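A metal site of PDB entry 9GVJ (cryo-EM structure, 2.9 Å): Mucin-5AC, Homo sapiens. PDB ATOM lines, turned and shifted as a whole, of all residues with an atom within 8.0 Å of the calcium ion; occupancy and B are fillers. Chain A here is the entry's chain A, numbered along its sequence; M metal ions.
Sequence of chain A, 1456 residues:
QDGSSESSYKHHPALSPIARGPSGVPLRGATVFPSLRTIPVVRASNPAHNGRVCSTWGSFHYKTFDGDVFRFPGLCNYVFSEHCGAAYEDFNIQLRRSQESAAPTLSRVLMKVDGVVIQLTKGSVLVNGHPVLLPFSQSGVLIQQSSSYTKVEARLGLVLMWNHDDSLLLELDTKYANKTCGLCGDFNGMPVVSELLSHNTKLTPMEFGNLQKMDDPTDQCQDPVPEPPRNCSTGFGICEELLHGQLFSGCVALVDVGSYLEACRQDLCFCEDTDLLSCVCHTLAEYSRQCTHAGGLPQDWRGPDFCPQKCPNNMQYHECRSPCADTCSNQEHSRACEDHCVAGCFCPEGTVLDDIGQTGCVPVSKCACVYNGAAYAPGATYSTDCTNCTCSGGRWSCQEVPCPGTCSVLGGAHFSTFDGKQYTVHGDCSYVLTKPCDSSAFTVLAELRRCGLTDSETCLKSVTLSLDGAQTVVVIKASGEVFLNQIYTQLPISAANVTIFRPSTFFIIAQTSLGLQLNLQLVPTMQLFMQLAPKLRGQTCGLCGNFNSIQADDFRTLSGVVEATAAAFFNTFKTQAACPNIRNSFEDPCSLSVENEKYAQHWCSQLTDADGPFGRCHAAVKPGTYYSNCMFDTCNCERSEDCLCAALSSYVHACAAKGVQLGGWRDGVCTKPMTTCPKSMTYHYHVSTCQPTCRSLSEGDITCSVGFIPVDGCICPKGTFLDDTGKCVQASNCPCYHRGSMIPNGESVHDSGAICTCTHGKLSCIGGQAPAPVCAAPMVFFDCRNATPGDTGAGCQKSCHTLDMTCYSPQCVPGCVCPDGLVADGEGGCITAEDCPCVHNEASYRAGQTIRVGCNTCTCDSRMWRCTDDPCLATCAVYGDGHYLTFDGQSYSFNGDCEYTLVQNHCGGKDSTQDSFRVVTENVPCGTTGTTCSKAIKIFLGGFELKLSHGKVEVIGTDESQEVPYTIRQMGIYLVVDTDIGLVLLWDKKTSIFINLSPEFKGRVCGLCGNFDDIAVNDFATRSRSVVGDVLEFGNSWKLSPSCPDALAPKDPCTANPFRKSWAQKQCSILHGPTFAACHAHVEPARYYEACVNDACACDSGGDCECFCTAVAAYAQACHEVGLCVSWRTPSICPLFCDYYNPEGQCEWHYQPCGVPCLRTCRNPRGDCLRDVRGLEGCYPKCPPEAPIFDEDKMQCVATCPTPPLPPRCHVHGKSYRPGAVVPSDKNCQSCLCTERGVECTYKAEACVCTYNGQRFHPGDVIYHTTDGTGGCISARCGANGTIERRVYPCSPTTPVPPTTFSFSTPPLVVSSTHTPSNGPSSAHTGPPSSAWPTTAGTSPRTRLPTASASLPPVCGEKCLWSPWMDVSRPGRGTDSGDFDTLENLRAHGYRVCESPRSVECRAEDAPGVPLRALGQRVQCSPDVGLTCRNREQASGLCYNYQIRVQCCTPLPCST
OD1 of Asp 66 is in hydrogen-bond range of N of Asn 188, at 3.1 Å.
O of Asp 186 lies close to N of Asn 178, 3.5 Å away.
OD1 of Asp 66 sits at hydrogen-bond distance from N of Gly 189 (2.8 Å).
The backbone NH (N) of Asp 66 lies close to the side-chain hydroxyl (OG1) of Thr 64 (3.4 Å).
Six residues have an atom within 4 Å of the calcium ion: Asp 66, Asp 186, Asn 188, Met 190, Val 193 and Glu 195.
The calcium ion is bound by O of Val 193, at 2.3 Å.
The calcium ion is bound by OD1 of Asn 188 (2.3 Å).
The calcium ion is bound by the side-chain carboxylate (OE2) of Glu 195.
The backbone carbonyl oxygen (O) of Met 190 is bound to the calcium ion.
OD1 of Asp 186 is bound to the calcium ion, at 2.7 Å.
Slightly farther from the calcium ion lies the side-chain amide nitrogen (ND2) of Asn 188 (3.0 Å).
Slightly farther from the calcium ion lies OD2 of Asp 66 (3.0 Å).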
ATOM      1  N   THR A  64       5.239 -13.818 -26.918  1.00  0.00           N
ATOM      2  CA  THR A  64       6.169 -14.871 -27.274  1.00  0.00           C
ATOM      3  C   THR A  64       5.421 -16.047 -27.898  1.00  0.00           C
ATOM      4  O   THR A  64       4.180 -16.086 -27.921  1.00  0.00           O
ATOM      5  CB  THR A  64       6.959 -15.319 -26.042  1.00  0.00           C
ATOM      6  OG1 THR A  64       6.085 -16.004 -25.136  1.00  0.00           O
ATOM      7  CG2 THR A  64       7.583 -14.120 -25.345  1.00  0.00           C
ATOM      8  N   PHE A  65       6.175 -17.002 -28.439  1.00  0.00           N
ATOM      9  CA  PHE A  65       5.556 -18.186 -29.014  1.00  0.00           C
ATOM     10  C   PHE A  65       4.789 -18.990 -27.962  1.00  0.00           C
ATOM     11  O   PHE A  65       3.825 -19.678 -28.294  1.00  0.00           O
ATOM     12  CB  PHE A  65       6.610 -19.077 -29.672  1.00  0.00           C
ATOM     13  CG  PHE A  65       7.132 -18.541 -30.966  1.00  0.00           C
ATOM     14  CD1 PHE A  65       6.317 -18.483 -32.086  1.00  0.00           C
ATOM     15  CD2 PHE A  65       8.439 -18.098 -31.072  1.00  0.00           C
ATOM     16  CE1 PHE A  65       6.798 -17.984 -33.281  1.00  0.00           C
ATOM     17  CE2 PHE A  65       8.919 -17.599 -32.267  1.00  0.00           C
ATOM     18  CZ  PHE A  65       8.104 -17.540 -33.376  1.00  0.00           C
ATOM     19  N   ASP A  66       5.206 -18.904 -26.707  1.00  0.00           N
ATOM     20  CA  ASP A  66       4.598 -19.686 -25.635  1.00  0.00           C
ATOM     21  C   ASP A  66       3.398 -18.998 -24.999  1.00  0.00           C
ATOM     22  O   ASP A  66       2.784 -19.576 -24.089  1.00  0.00           O
ATOM     23  CB  ASP A  66       5.653 -20.005 -24.571  1.00  0.00           C
ATOM     24  CG  ASP A  66       6.781 -20.856 -25.111  1.00  0.00           C
ATOM     25  OD1 ASP A  66       6.561 -21.568 -26.111  1.00  0.00           O
ATOM     26  OD2 ASP A  66       7.887 -20.802 -24.550  1.00  0.00           O
ATOM     27  N   ASN A 178      11.344 -25.538 -29.581  1.00  0.00           N
ATOM     28  CA  ASN A 178      12.423 -25.797 -28.630  1.00  0.00           C
ATOM     29  C   ASN A 178      13.793 -25.525 -29.218  1.00  0.00           C
ATOM     30  O   ASN A 178      14.796 -26.071 -28.738  1.00  0.00           O
ATOM     31  CB  ASN A 178      12.349 -27.231 -28.096  1.00  0.00           C
ATOM     32  CG  ASN A 178      12.762 -27.337 -26.642  1.00  0.00           C
ATOM     33  OD1 ASN A 178      13.153 -26.354 -26.019  1.00  0.00           O
ATOM     34  ND2 ASN A 178      12.678 -28.546 -26.088  1.00  0.00           N
ATOM     35  N   GLY A 185      10.779 -15.814 -27.362  1.00  0.00           N
ATOM     36  CA  GLY A 185      10.854 -16.990 -26.526  1.00  0.00           C
ATOM     37  C   GLY A 185      11.554 -18.160 -27.187  1.00  0.00           C
ATOM     38  O   GLY A 185      12.005 -18.105 -28.336  1.00  0.00           O
ATOM     39  N   ASP A 186      11.650 -19.244 -26.418  1.00  0.00           N
ATOM     40  CA  ASP A 186      12.343 -20.441 -26.864  1.00  0.00           C
ATOM     41  C   ASP A 186      11.425 -21.454 -27.556  1.00  0.00           C
ATOM     42  O   ASP A 186      11.911 -22.494 -28.015  1.00  0.00           O
ATOM     43  CB  ASP A 186      13.053 -21.110 -25.684  1.00  0.00           C
ATOM     44  CG  ASP A 186      12.095 -21.787 -24.730  1.00  0.00           C
ATOM     45  OD1 ASP A 186      11.046 -21.185 -24.410  1.00  0.00           O
ATOM     46  OD2 ASP A 186      12.385 -22.914 -24.285  1.00  0.00           O
ATOM     47  N   PHE A 187      10.126 -21.167 -27.627  1.00  0.00           N
ATOM     48  CA  PHE A 187       9.176 -21.948 -28.436  1.00  0.00           C
ATOM     49  C   PHE A 187       9.147 -23.416 -27.993  1.00  0.00           C
ATOM     50  O   PHE A 187       9.456 -24.330 -28.751  1.00  0.00           O
ATOM     51  CB  PHE A 187       9.536 -21.825 -29.928  1.00  0.00           C
ATOM     52  CG  PHE A 187       8.482 -22.342 -30.866  1.00  0.00           C
ATOM     53  CD1 PHE A 187       7.215 -22.688 -30.409  1.00  0.00           C
ATOM     54  CD2 PHE A 187       8.756 -22.484 -32.214  1.00  0.00           C
ATOM     55  CE1 PHE A 187       6.264 -23.165 -31.276  1.00  0.00           C
ATOM     56  CE2 PHE A 187       7.806 -22.962 -33.090  1.00  0.00           C
ATOM     57  CZ  PHE A 187       6.546 -23.300 -32.624  1.00  0.00           C
ATOM     58  N   ASN A 188       8.747 -23.613 -26.733  1.00  0.00           N
ATOM     59  CA  ASN A 188       8.618 -24.959 -26.184  1.00  0.00           C
ATOM     60  C   ASN A 188       7.256 -25.199 -25.527  1.00  0.00           C
ATOM     61  O   ASN A 188       7.073 -26.252 -24.889  1.00  0.00           O
ATOM     62  CB  ASN A 188       9.728 -25.247 -25.176  1.00  0.00           C
ATOM     63  CG  ASN A 188       9.716 -24.296 -23.997  1.00  0.00           C
ATOM     64  OD1 ASN A 188       9.030 -23.282 -24.009  1.00  0.00           O
ATOM     65  ND2 ASN A 188      10.493 -24.627 -22.969  1.00  0.00           N
ATOM     66  N   GLY A 189       6.309 -24.278 -25.658  1.00  0.00           N
ATOM     67  CA  GLY A 189       4.978 -24.465 -25.113  1.00  0.00           C
ATOM     68  C   GLY A 189       4.810 -24.109 -23.658  1.00  0.00           C
ATOM     69  O   GLY A 189       3.708 -24.315 -23.120  1.00  0.00           O
ATOM     70  N   MET A 190       5.847 -23.594 -22.996  1.00  0.00           N
ATOM     71  CA  MET A 190       5.762 -23.211 -21.593  1.00  0.00           C
ATOM     72  C   MET A 190       6.179 -21.757 -21.454  1.00  0.00           C
ATOM     73  O   MET A 190       7.269 -21.379 -21.907  1.00  0.00           O
ATOM     74  CB  MET A 190       6.645 -24.128 -20.731  1.00  0.00           C
ATOM     75  CG  MET A 190       6.242 -25.603 -20.836  1.00  0.00           C
ATOM     76  SD  MET A 190       7.564 -26.796 -20.558  1.00  0.00           S
ATOM     77  CE  MET A 190       8.742 -25.811 -19.646  1.00  0.00           C
ATOM     78  N   PRO A 191       5.353 -20.914 -20.822  1.00  0.00           N
ATOM     79  CA  PRO A 191       5.546 -19.456 -20.968  1.00  0.00           C
ATOM     80  C   PRO A 191       6.774 -18.915 -20.261  1.00  0.00           C
ATOM     81  O   PRO A 191       7.513 -18.116 -20.841  1.00  0.00           O
ATOM     82  CB  PRO A 191       4.253 -18.872 -20.385  1.00  0.00           C
ATOM     83  CG  PRO A 191       3.288 -20.025 -20.301  1.00  0.00           C
ATOM     84  CD  PRO A 191       4.131 -21.230 -20.058  1.00  0.00           C
ATOM     85  N   VAL A 192       7.012 -19.319 -19.017  1.00  0.00           N
ATOM     86  CA  VAL A 192       8.030 -18.696 -18.175  1.00  0.00           C
ATOM     87  C   VAL A 192       9.360 -19.422 -18.263  1.00  0.00           C
ATOM     88  O   VAL A 192      10.412 -18.797 -18.338  1.00  0.00           O
ATOM     89  CB  VAL A 192       7.526 -18.593 -16.723  1.00  0.00           C
ATOM     90  CG1 VAL A 192       8.689 -18.618 -15.742  1.00  0.00           C
ATOM     91  CG2 VAL A 192       6.695 -17.344 -16.523  1.00  0.00           C
ATOM     92  N   VAL A 193       9.333 -20.756 -18.248  1.00  0.00           N
ATOM     93  CA  VAL A 193      10.559 -21.541 -18.172  1.00  0.00           C
ATOM     94  C   VAL A 193      11.399 -21.327 -19.425  1.00  0.00           C
ATOM     95  O   VAL A 193      10.873 -21.282 -20.554  1.00  0.00           O
ATOM     96  CB  VAL A 193      10.224 -23.033 -17.972  1.00  0.00           C
ATOM     97  CG1 VAL A 193      11.467 -23.887 -18.121  1.00  0.00           C
ATOM     98  CG2 VAL A 193       9.564 -23.245 -16.624  1.00  0.00           C
ATOM     99  N   SER A 194      12.703 -21.170 -19.231  1.00  0.00           N
ATOM    100  CA  SER A 194      13.745 -21.040 -20.256  1.00  0.00           C
ATOM    101  C   SER A 194      13.738 -19.685 -20.947  1.00  0.00           C
ATOM    102  O   SER A 194      14.563 -19.465 -21.847  1.00  0.00           O
ATOM    103  CB  SER A 194      13.668 -22.149 -21.312  1.00  0.00           C
ATOM    104  OG  SER A 194      13.927 -23.413 -20.737  1.00  0.00           O
ATOM    105  N   GLU A 195      12.839 -18.772 -20.584  1.00  0.00           N
ATOM    106  CA  GLU A 195      12.851 -17.422 -21.119  1.00  0.00           C
ATOM    107  C   GLU A 195      13.055 -16.366 -20.042  1.00  0.00           C
ATOM    108  O   GLU A 195      13.816 -15.415 -20.247  1.00  0.00           O
ATOM    109  CB  GLU A 195      11.546 -17.118 -21.871  1.00  0.00           C
ATOM    110  CG  GLU A 195      11.276 -18.063 -23.029  1.00  0.00           C
ATOM    111  CD  GLU A 195       9.824 -18.484 -23.097  1.00  0.00           C
ATOM    112  OE1 GLU A 195       9.012 -17.720 -23.651  1.00  0.00           O
ATOM    113  OE2 GLU A 195       9.497 -19.583 -22.597  1.00  0.00           O
ATOM    114  N   LEU A 196      12.389 -16.519 -18.892  1.00  0.00           N
ATOM    115  CA  LEU A 196      12.525 -15.593 -17.772  1.00  0.00           C
ATOM    116  C   LEU A 196      13.465 -16.124 -16.704  1.00  0.00           C
ATOM    117  O   LEU A 196      13.503 -15.578 -15.593  1.00  0.00           O
ATOM    118  CB  LEU A 196      11.158 -15.291 -17.175  1.00  0.00           C
ATOM    119  CG  LEU A 196      10.174 -14.535 -18.086  1.00  0.00           C
ATOM    120  CD1 LEU A 196       8.980 -14.031 -17.311  1.00  0.00           C
ATOM    121  CD2 LEU A 196      10.877 -13.397 -18.802  1.00  0.00           C
ATOM    122  N   LEU A 197      14.212 -17.190 -17.003  1.00  0.00           N
ATOM    123  CA  LEU A 197      15.162 -17.789 -16.070  1.00  0.00           C
ATOM    124  C   LEU A 197      16.545 -17.760 -16.716  1.00  0.00           C
ATOM    125  O   LEU A 197      16.737 -18.329 -17.793  1.00  0.00           O
ATOM    126  CB  LEU A 197      14.770 -19.219 -15.721  1.00  0.00           C
ATOM    127  CG  LEU A 197      13.278 -19.524 -15.552  1.00  0.00           C
ATOM    128  CD1 LEU A 197      13.037 -21.026 -15.511  1.00  0.00           C
ATOM    129  CD2 LEU A 197      12.731 -18.871 -14.297  1.00  0.00           C
HETATM  130 CA    CA M   1       9.554 -21.861 -22.293  1.00  0.00          CA
